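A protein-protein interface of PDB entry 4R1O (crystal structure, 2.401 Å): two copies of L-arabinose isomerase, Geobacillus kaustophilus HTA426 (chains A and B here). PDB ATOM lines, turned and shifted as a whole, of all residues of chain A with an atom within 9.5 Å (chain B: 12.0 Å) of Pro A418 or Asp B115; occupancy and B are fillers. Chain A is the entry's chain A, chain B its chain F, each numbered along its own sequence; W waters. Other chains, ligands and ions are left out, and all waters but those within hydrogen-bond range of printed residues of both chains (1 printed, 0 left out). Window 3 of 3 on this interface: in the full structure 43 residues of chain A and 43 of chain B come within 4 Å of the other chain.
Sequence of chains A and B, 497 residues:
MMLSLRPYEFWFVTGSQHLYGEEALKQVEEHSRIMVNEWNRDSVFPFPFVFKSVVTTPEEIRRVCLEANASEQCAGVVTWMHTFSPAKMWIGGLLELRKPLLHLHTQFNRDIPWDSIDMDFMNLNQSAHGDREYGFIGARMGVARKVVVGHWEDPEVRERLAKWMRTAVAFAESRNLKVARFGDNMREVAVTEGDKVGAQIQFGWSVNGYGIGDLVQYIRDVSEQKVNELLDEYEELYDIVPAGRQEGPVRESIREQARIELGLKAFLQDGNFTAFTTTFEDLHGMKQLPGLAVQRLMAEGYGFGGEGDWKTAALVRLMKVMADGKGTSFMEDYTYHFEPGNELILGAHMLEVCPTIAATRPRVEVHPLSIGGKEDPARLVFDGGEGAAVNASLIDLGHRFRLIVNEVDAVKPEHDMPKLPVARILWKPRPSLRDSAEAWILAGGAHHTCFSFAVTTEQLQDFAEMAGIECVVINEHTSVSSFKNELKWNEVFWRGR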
ATOM      1  N   ARG A 363      17.537  33.173  37.867  1.00  0.00           N
ATOM      2  CA  ARG A 363      16.353  33.442  37.077  1.00  0.00           C
ATOM      3  C   ARG A 363      15.337  32.339  37.323  1.00  0.00           C
ATOM      4  O   ARG A 363      15.704  31.161  37.404  1.00  0.00           O
ATOM      5  CB  ARG A 363      16.678  33.574  35.585  1.00  0.00           C
ATOM      6  CG  ARG A 363      15.485  34.063  34.749  1.00  0.00           C
ATOM      7  CD  ARG A 363      15.918  34.832  33.484  1.00  0.00           C
ATOM      8  NE  ARG A 363      16.527  33.945  32.505  1.00  0.00           N
ATOM      9  CZ  ARG A 363      16.163  33.881  31.228  1.00  0.00           C
ATOM     10  NH1 ARG A 363      15.197  34.672  30.772  1.00  0.00           N
ATOM     11  NH2 ARG A 363      16.767  33.030  30.406  1.00  0.00           N
ATOM     12  N   GLU A 365      12.750  30.227  35.699  1.00  0.00           N
ATOM     13  CA  GLU A 365      12.353  29.754  34.369  1.00  0.00           C
ATOM     14  C   GLU A 365      11.416  28.562  34.483  1.00  0.00           C
ATOM     15  O   GLU A 365      11.316  27.946  35.537  1.00  0.00           O
ATOM     16  CB  GLU A 365      13.592  29.379  33.554  1.00  0.00           C
ATOM     17  CG  GLU A 365      14.692  30.428  33.610  1.00  0.00           C
ATOM     18  CD  GLU A 365      15.885  30.096  32.716  1.00  0.00           C
ATOM     19  OE1 GLU A 365      15.923  28.987  32.121  1.00  0.00           O
ATOM     20  OE2 GLU A 365      16.789  30.953  32.608  1.00  0.00           O
ATOM     21  N   HIS A 367      10.447  24.911  32.342  1.00  0.00           N
ATOM     22  CA  HIS A 367      10.847  24.064  31.226  1.00  0.00           C
ATOM     23  C   HIS A 367      10.191  22.709  31.406  1.00  0.00           C
ATOM     24  O   HIS A 367       9.735  22.390  32.505  1.00  0.00           O
ATOM     25  CB  HIS A 367      12.376  23.900  31.172  1.00  0.00           C
ATOM     26  CG  HIS A 367      13.128  25.170  30.903  1.00  0.00           C
ATOM     27  ND1 HIS A 367      13.374  25.639  29.627  1.00  0.00           N
ATOM     28  CD2 HIS A 367      13.715  26.054  31.748  1.00  0.00           C
ATOM     29  CE1 HIS A 367      14.065  26.765  29.698  1.00  0.00           C
ATOM     30  NE2 HIS A 367      14.288  27.037  30.972  1.00  0.00           N
ATOM     31  N   VAL A 381      17.407  29.159  37.799  1.00  0.00           N
ATOM     32  CA  VAL A 381      18.543  28.860  36.949  1.00  0.00           C
ATOM     33  C   VAL A 381      19.639  29.900  37.155  1.00  0.00           C
ATOM     34  O   VAL A 381      19.375  31.100  37.176  1.00  0.00           O
ATOM     35  CB  VAL A 381      18.128  28.840  35.471  1.00  0.00           C
ATOM     36  CG1 VAL A 381      19.321  28.480  34.582  1.00  0.00           C
ATOM     37  CG2 VAL A 381      16.983  27.854  35.260  1.00  0.00           C
ATOM     38  N   ASP A 383      24.416  30.306  37.334  1.00  0.00           N
ATOM     39  CA  ASP A 383      25.727  29.679  37.358  1.00  0.00           C
ATOM     40  C   ASP A 383      26.294  29.807  38.755  1.00  0.00           C
ATOM     41  O   ASP A 383      26.206  30.870  39.371  1.00  0.00           O
ATOM     42  CB  ASP A 383      26.679  30.369  36.387  1.00  0.00           C
ATOM     43  CG  ASP A 383      26.244  30.240  34.952  1.00  0.00           C
ATOM     44  OD1 ASP A 383      26.057  29.099  34.483  1.00  0.00           O
ATOM     45  OD2 ASP A 383      26.094  31.287  34.292  1.00  0.00           O
ATOM     46  N   GLU A 414      33.199  29.799  31.162  1.00  0.00           N
ATOM     47  CA  GLU A 414      33.733  30.590  30.061  1.00  0.00           C
ATOM     48  C   GLU A 414      32.719  30.707  28.913  1.00  0.00           C
ATOM     49  O   GLU A 414      32.864  31.560  28.041  1.00  0.00           O
ATOM     50  CB  GLU A 414      35.039  29.981  29.549  1.00  0.00           C
ATOM     51  CG  GLU A 414      36.258  30.324  30.400  1.00  0.00           C
ATOM     52  CD  GLU A 414      37.442  29.416  30.113  1.00  0.00           C
ATOM     53  OE1 GLU A 414      38.433  29.462  30.876  1.00  0.00           O
ATOM     54  OE2 GLU A 414      37.378  28.648  29.126  1.00  0.00           O
ATOM     55  N   HIS A 415      31.697  29.849  28.918  1.00  0.00           N
ATOM     56  CA  HIS A 415      30.670  29.874  27.881  1.00  0.00           C
ATOM     57  C   HIS A 415      29.272  29.825  28.467  1.00  0.00           C
ATOM     58  O   HIS A 415      29.052  29.234  29.527  1.00  0.00           O
ATOM     59  CB  HIS A 415      30.847  28.699  26.921  1.00  0.00           C
ATOM     60  CG  HIS A 415      32.179  28.671  26.250  1.00  0.00           C
ATOM     61  ND1 HIS A 415      33.256  27.983  26.767  1.00  0.00           N
ATOM     62  CD2 HIS A 415      32.620  29.271  25.119  1.00  0.00           C
ATOM     63  CE1 HIS A 415      34.300  28.148  25.973  1.00  0.00           C
ATOM     64  NE2 HIS A 415      33.940  28.928  24.969  1.00  0.00           N
ATOM     65  N   ASP A 416      28.323  30.446  27.775  1.00  0.00           N
ATOM     66  CA  ASP A 416      26.926  30.323  28.155  1.00  0.00           C
ATOM     67  C   ASP A 416      26.456  28.927  27.838  1.00  0.00           C
ATOM     68  O   ASP A 416      26.970  28.275  26.928  1.00  0.00           O
ATOM     69  CB  ASP A 416      26.053  31.333  27.409  1.00  0.00           C
ATOM     70  CG  ASP A 416      26.143  32.714  28.001  1.00  0.00           C
ATOM     71  OD1 ASP A 416      26.664  32.835  29.132  1.00  0.00           O
ATOM     72  OD2 ASP A 416      25.686  33.671  27.344  1.00  0.00           O
ATOM     73  N   MET A 417      25.480  28.463  28.606  1.00  0.00           N
ATOM     74  CA  MET A 417      24.828  27.198  28.330  1.00  0.00           C
ATOM     75  C   MET A 417      23.350  27.496  28.151  1.00  0.00           C
ATOM     76  O   MET A 417      22.533  27.156  29.010  1.00  0.00           O
ATOM     77  CB  MET A 417      25.083  26.213  29.467  1.00  0.00           C
ATOM     78  CG  MET A 417      26.510  25.654  29.464  1.00  0.00           C
ATOM     79  SD  MET A 417      26.973  24.776  30.976  1.00  0.00           S
ATOM     80  CE  MET A 417      27.527  26.139  31.997  1.00  0.00           C
ATOM     81  N   PRO A 418      23.007  28.144  27.019  1.00  0.00           N
ATOM     82  CA  PRO A 418      21.687  28.732  26.764  1.00  0.00           C
ATOM     83  C   PRO A 418      20.556  27.711  26.702  1.00  0.00           C
ATOM     84  O   PRO A 418      19.397  28.057  26.929  1.00  0.00           O
ATOM     85  CB  PRO A 418      21.866  29.418  25.408  1.00  0.00           C
ATOM     86  CG  PRO A 418      22.934  28.635  24.735  1.00  0.00           C
ATOM     87  CD  PRO A 418      23.882  28.241  25.836  1.00  0.00           C
ATOM     88  N   LYS A 419      20.884  26.459  26.427  1.00  0.00           N
ATOM     89  CA  LYS A 419      19.847  25.453  26.264  1.00  0.00           C
ATOM     90  C   LYS A 419      19.705  24.576  27.505  1.00  0.00           C
ATOM     91  O   LYS A 419      18.840  23.698  27.555  1.00  0.00           O
ATOM     92  CB  LYS A 419      20.135  24.608  25.025  1.00  0.00           C
ATOM     93  CG  LYS A 419      20.200  25.417  23.731  1.00  0.00           C
ATOM     94  CD  LYS A 419      18.896  26.177  23.498  1.00  0.00           C
ATOM     95  CE  LYS A 419      17.690  25.233  23.382  1.00  0.00           C
ATOM     96  NZ  LYS A 419      16.377  25.952  23.507  1.00  0.00           N
ATOM     97  N   LEU A 420      20.547  24.824  28.506  1.00  0.00           N
ATOM     98  CA  LEU A 420      20.563  24.008  29.715  1.00  0.00           C
ATOM     99  C   LEU A 420      19.605  24.571  30.745  1.00  0.00           C
ATOM    100  O   LEU A 420      19.879  25.597  31.344  1.00  0.00           O
ATOM    101  CB  LEU A 420      21.972  23.947  30.298  1.00  0.00           C
ATOM    102  CG  LEU A 420      22.165  23.117  31.569  1.00  0.00           C
ATOM    103  CD1 LEU A 420      21.732  21.695  31.318  1.00  0.00           C
ATOM    104  CD2 LEU A 420      23.631  23.148  32.007  1.00  0.00           C
ATOM    105  N   PRO A 421      18.486  23.880  30.982  1.00  0.00           N
ATOM    106  CA  PRO A 421      17.401  24.447  31.788  1.00  0.00           C
ATOM    107  C   PRO A 421      17.561  24.262  33.300  1.00  0.00           C
ATOM    108  O   PRO A 421      16.563  24.407  34.015  1.00  0.00           O
ATOM    109  CB  PRO A 421      16.191  23.649  31.308  1.00  0.00           C
ATOM    110  CG  PRO A 421      16.760  22.292  31.055  1.00  0.00           C
ATOM    111  CD  PRO A 421      18.179  22.503  30.552  1.00  0.00           C
ATOM    112  N   VAL A 422      18.765  23.953  33.786  1.00  0.00           N
ATOM    113  CA  VAL A 422      18.968  23.857  35.231  1.00  0.00           C
ATOM    114  C   VAL A 422      20.149  24.645  35.747  1.00  0.00           C
ATOM    115  O   VAL A 422      21.117  24.886  35.034  1.00  0.00           O
ATOM    116  CB  VAL A 422      19.115  22.404  35.730  1.00  0.00           C
ATOM    117  CG1 VAL A 422      17.892  21.592  35.360  1.00  0.00           C
ATOM    118  CG2 VAL A 422      20.402  21.770  35.203  1.00  0.00           C
ATOM    119  N   ARG A 424      23.540  25.208  37.654  1.00  0.00           N
ATOM    120  CA  ARG A 424      24.724  24.362  37.630  1.00  0.00           C
ATOM    121  C   ARG A 424      25.966  25.119  38.102  1.00  0.00           C
ATOM    122  O   ARG A 424      25.983  26.348  38.160  1.00  0.00           O
ATOM    123  CB  ARG A 424      24.948  23.778  36.224  1.00  0.00           C
ATOM    124  CG  ARG A 424      25.733  24.671  35.233  1.00  0.00           C
ATOM    125  CD  ARG A 424      25.068  26.037  34.968  1.00  0.00           C
ATOM    126  NE  ARG A 424      23.755  25.933  34.333  1.00  0.00           N
ATOM    127  CZ  ARG A 424      23.319  26.758  33.380  1.00  0.00           C
ATOM    128  NH1 ARG A 424      22.106  26.591  32.861  1.00  0.00           N
ATOM    129  NH2 ARG A 424      24.096  27.748  32.939  1.00  0.00           N
ATOM    130  N   ASN B 109      31.620  11.512  24.794  1.00  0.00           N
ATOM    131  CA  ASN B 109      32.134  12.788  24.315  1.00  0.00           C
ATOM    132  C   ASN B 109      33.239  13.269  25.230  1.00  0.00           C
ATOM    133  O   ASN B 109      33.181  13.055  26.436  1.00  0.00           O
ATOM    134  CB  ASN B 109      31.019  13.822  24.331  1.00  0.00           C
ATOM    135  CG  ASN B 109      30.412  13.979  25.719  1.00  0.00           C
ATOM    136  OD1 ASN B 109      29.749  13.066  26.216  1.00  0.00           O
ATOM    137  ND2 ASN B 109      30.658  15.122  26.359  1.00  0.00           N
ATOM    138  N   ASP B 111      34.345  16.743  25.378  1.00  0.00           N
ATOM    139  CA  ASP B 111      34.000  18.070  25.867  1.00  0.00           C
ATOM    140  C   ASP B 111      32.512  18.280  26.098  1.00  0.00           C
ATOM    141  O   ASP B 111      31.666  17.646  25.459  1.00  0.00           O
ATOM    142  CB  ASP B 111      34.478  19.132  24.881  1.00  0.00           C
ATOM    143  CG  ASP B 111      35.972  19.142  24.726  1.00  0.00           C
ATOM    144  OD1 ASP B 111      36.645  18.391  25.455  1.00  0.00           O
ATOM    145  OD2 ASP B 111      36.477  19.899  23.878  1.00  0.00           O
ATOM    146  N   ILE B 112      32.202  19.197  27.014  1.00  0.00           N
ATOM    147  CA  ILE B 112      30.847  19.707  27.145  1.00  0.00           C
ATOM    148  C   ILE B 112      30.547  20.627  25.973  1.00  0.00           C
ATOM    149  O   ILE B 112      31.201  21.653  25.807  1.00  0.00           O
ATOM    150  CB  ILE B 112      30.650  20.524  28.437  1.00  0.00           C
ATOM    151  CG1 ILE B 112      30.769  19.634  29.662  1.00  0.00           C
ATOM    152  CG2 ILE B 112      29.289  21.216  28.413  1.00  0.00           C
ATOM    153  CD1 ILE B 112      30.635  20.382  30.949  1.00  0.00           C
ATOM    154  N   PRO B 113      29.542  20.268  25.162  1.00  0.00           N
ATOM    155  CA  PRO B 113      29.122  21.122  24.049  1.00  0.00           C
ATOM    156  C   PRO B 113      28.289  22.270  24.609  1.00  0.00           C
ATOM    157  O   PRO B 113      27.064  22.194  24.655  1.00  0.00           O
ATOM    158  CB  PRO B 113      28.263  20.176  23.204  1.00  0.00           C
ATOM    159  CG  PRO B 113      27.663  19.238  24.201  1.00  0.00           C
ATOM    160  CD  PRO B 113      28.700  19.064  25.289  1.00  0.00           C
ATOM    161  N   TRP B 114      28.969  23.316  25.050  1.00  0.00           N
ATOM    162  CA  TRP B 114      28.341  24.446  25.742  1.00  0.00           C
ATOM    163  C   TRP B 114      27.061  24.986  25.115  1.00  0.00           C
ATOM    164  O   TRP B 114      26.051  25.159  25.798  1.00  0.00           O
ATOM    165  CB  TRP B 114      29.358  25.581  25.909  1.00  0.00           C
ATOM    166  CG  TRP B 114      30.673  25.087  26.467  1.00  0.00           C
ATOM    167  CD1 TRP B 114      31.828  24.869  25.769  1.00  0.00           C
ATOM    168  CD2 TRP B 114      30.954  24.718  27.831  1.00  0.00           C
ATOM    169  NE1 TRP B 114      32.812  24.406  26.612  1.00  0.00           N
ATOM    170  CE2 TRP B 114      32.303  24.304  27.883  1.00  0.00           C
ATOM    171  CE3 TRP B 114      30.197  24.704  29.013  1.00  0.00           C
ATOM    172  CZ2 TRP B 114      32.917  23.881  29.074  1.00  0.00           C
ATOM    173  CZ3 TRP B 114      30.805  24.281  30.198  1.00  0.00           C
ATOM    174  CH2 TRP B 114      32.155  23.881  30.214  1.00  0.00           C
ATOM    175  N   ASP B 115      27.100  25.245  23.816  1.00  0.00           N
ATOM    176  CA  ASP B 115      26.005  25.949  23.159  1.00  0.00           C
ATOM    177  C   ASP B 115      24.741  25.106  22.986  1.00  0.00           C
ATOM    178  O   ASP B 115      23.675  25.640  22.692  1.00  0.00           O
ATOM    179  CB  ASP B 115      26.465  26.510  21.804  1.00  0.00           C
ATOM    180  CG  ASP B 115      26.748  25.422  20.767  1.00  0.00           C
ATOM    181  OD1 ASP B 115      26.787  24.217  21.112  1.00  0.00           O
ATOM    182  OD2 ASP B 115      26.947  25.788  19.587  1.00  0.00           O
ATOM    183  N   SER B 116      24.854  23.794  23.156  1.00  0.00           N
ATOM    184  CA  SER B 116      23.720  22.931  22.872  1.00  0.00           C
ATOM    185  C   SER B 116      23.329  21.970  24.000  1.00  0.00           C
ATOM    186  O   SER B 116      22.294  21.310  23.910  1.00  0.00           O
ATOM    187  CB  SER B 116      23.975  22.138  21.600  1.00  0.00           C
ATOM    188  OG  SER B 116      24.821  21.048  21.875  1.00  0.00           O
ATOM    189  N   ILE B 117      24.136  21.881  25.053  1.00  0.00           N
ATOM    190  CA  ILE B 117      23.838  20.931  26.127  1.00  0.00           C
ATOM    191  C   ILE B 117      22.480  21.231  26.788  1.00  0.00           C
ATOM    192  O   ILE B 117      22.215  22.344  27.230  1.00  0.00           O
ATOM    193  CB  ILE B 117      24.959  20.851  27.170  1.00  0.00           C
ATOM    194  CG1 ILE B 117      24.538  19.950  28.335  1.00  0.00           C
ATOM    195  CG2 ILE B 117      25.319  22.246  27.683  1.00  0.00           C
ATOM    196  CD1 ILE B 117      25.627  19.765  29.389  1.00  0.00           C
ATOM    197  N   ASP B 118      21.615  20.225  26.800  1.00  0.00           N
ATOM    198  CA  ASP B 118      20.266  20.357  27.325  1.00  0.00           C
ATOM    199  C   ASP B 118      19.956  19.143  28.181  1.00  0.00           C
ATOM    200  O   ASP B 118      20.849  18.358  28.481  1.00  0.00           O
ATOM    201  CB  ASP B 118      19.246  20.480  26.186  1.00  0.00           C
ATOM    202  CG  ASP B 118      19.295  19.303  25.206  1.00  0.00           C
ATOM    203  OD1 ASP B 118      19.971  18.283  25.488  1.00  0.00           O
ATOM    204  OD2 ASP B 118      18.630  19.391  24.147  1.00  0.00           O
ATOM    205  N   MET B 119      18.694  18.974  28.558  1.00  0.00           N
ATOM    206  CA  MET B 119      18.329  17.901  29.476  1.00  0.00           C
ATOM    207  C   MET B 119      18.596  16.507  28.888  1.00  0.00           C
ATOM    208  O   MET B 119      19.017  15.603  29.605  1.00  0.00           O
ATOM    209  CB  MET B 119      16.872  18.043  29.934  1.00  0.00           C
ATOM    210  CG  MET B 119      16.617  17.497  31.334  1.00  0.00           C
ATOM    211  SD  MET B 119      17.809  18.132  32.533  1.00  0.00           S
ATOM    212  CE  MET B 119      17.520  16.994  33.891  1.00  0.00           C
ATOM    213  N   ASP B 120      18.365  16.338  27.587  1.00  0.00           N
ATOM    214  CA  ASP B 120      18.600  15.052  26.928  1.00  0.00           C
ATOM    215  C   ASP B 120      20.064  14.615  26.968  1.00  0.00           C
ATOM    216  O   ASP B 120      20.366  13.437  27.096  1.00  0.00           O
ATOM    217  CB  ASP B 120      18.109  15.080  25.473  1.00  0.00           C
ATOM    218  CG  ASP B 120      16.610  14.877  25.369  1.00  0.00           C
ATOM    219  OD1 ASP B 120      16.032  14.295  26.311  1.00  0.00           O
ATOM    220  OD2 ASP B 120      16.013  15.300  24.362  1.00  0.00           O
ATOM    221  N   PHE B 121      20.965  15.576  26.840  1.00  0.00           N
ATOM    222  CA  PHE B 121      22.383  15.308  26.948  1.00  0.00           C
ATOM    223  C   PHE B 121      22.744  14.984  28.411  1.00  0.00           C
ATOM    224  O   PHE B 121      23.646  14.193  28.666  1.00  0.00           O
ATOM    225  CB  PHE B 121      23.165  16.530  26.441  1.00  0.00           C
ATOM    226  CG  PHE B 121      24.646  16.314  26.319  1.00  0.00           C
ATOM    227  CD1 PHE B 121      25.473  16.387  27.435  1.00  0.00           C
ATOM    228  CD2 PHE B 121      25.224  16.087  25.077  1.00  0.00           C
ATOM    229  CE1 PHE B 121      26.850  16.209  27.315  1.00  0.00           C
ATOM    230  CE2 PHE B 121      26.600  15.905  24.949  1.00  0.00           C
ATOM    231  CZ  PHE B 121      27.410  15.969  26.069  1.00  0.00           C
ATOM    232  N   MET B 122      22.038  15.600  29.359  1.00  0.00           N
ATOM    233  CA  MET B 122      22.332  15.419  30.777  1.00  0.00           C
ATOM    234  C   MET B 122      21.860  14.052  31.263  1.00  0.00           C
ATOM    235  O   MET B 122      22.445  13.474  32.185  1.00  0.00           O
ATOM    236  CB  MET B 122      21.686  16.527  31.620  1.00  0.00           C
ATOM    237  CG  MET B 122      22.220  17.938  31.367  1.00  0.00           C
ATOM    238  SD  MET B 122      23.678  18.371  32.354  1.00  0.00           S
ATOM    239  CE  MET B 122      22.900  18.906  33.887  1.00  0.00           C
HETATM  240  O   HOH W   1      23.169  24.906  26.175  1.00  0.00           O
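Of the 15 printed residues of chain A, 6 touch a printed residue of chain B.
Hydrophobic or aromatic side chains of chain B that line the printed part of chain A: Trp B114 and Met B122.
Among the printed residues, no Asp or Glu carboxylate lies within 4 Å of a Lys or Arg side-chain nitrogen of the other chain.
O of Leu A420 lies within hydrogen-bond range of NH1 of Arg A424, at 2.9 Å.
O of Ile B112 lies close to NE1 of Trp B114.
OD1 of Asp B118 sits close to N of Asp B120.
OD1 of Asp B118 lies within hydrogen-bond range of N of Phe B121, 3.2 Å away.
Water W1 lies within hydrogen-bond range of the backbone NH (N) of Lys A419 (2.8 Å), the backbone carbonyl oxygen (O) of Trp B114 (2.9 Å) and the backbone carbonyl oxygen (O) of Ile B117 (2.9 Å).
His A367 touches none of the printed residues of chain B.
Printed residues of chain B within 4 Å of His A415: Trp B114.
Asp A416 touches just one residue of chain B: Trp B114 (3.4 Å).
Met A417 touches one residue of chain B.
Printed residues of chain B within 4 Å of Lys A419: Asp B115, Ile B117 and Asp B118.
Asp B115 touches just these residues of chain A: Pro A418 (3.7 Å) and Lys A419 (3.6 Å).
Met B119 touches none of the printed residues of chain A.
Of the printed residues of chain A, Met B122 touches Leu A420 (3.8 Å).
The nearest residue of chain A that does not touch Asp B115 is Asp A416 (4.3 Å).
The nearest printed residue of chain A that does not touch Ile B117 is Met A417 (4.03 Å).
ND1 of His A415 touches CD1 of Trp B114, at 3.6 Å.
O of Trp B114 touches CA of Met A417 (3.5 Å).
Trp B114 touches Pro A418.
Asp B115 touches Pro A418 (O to CG, 3.7 Å).
Lys A419 touches Asp B115.
C of Lys A419 touches O of Ile B117 (3.4 Å).
Lys A419 touches Asp B118 (O to CB, 3.5 Å).
Met B122 touches Leu A420.
No position is printed for both chains.
Of the 10 pairs that touch across the chains among the printed residues, none has its exchanged pair printed and touching as well.
The backbone NH (N) of Leu A420 is in hydrogen-bond range of the backbone carbonyl oxygen (O) of Ile B117 (3.2 Å).
O of Asp A416 sits close to O of Trp B114.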
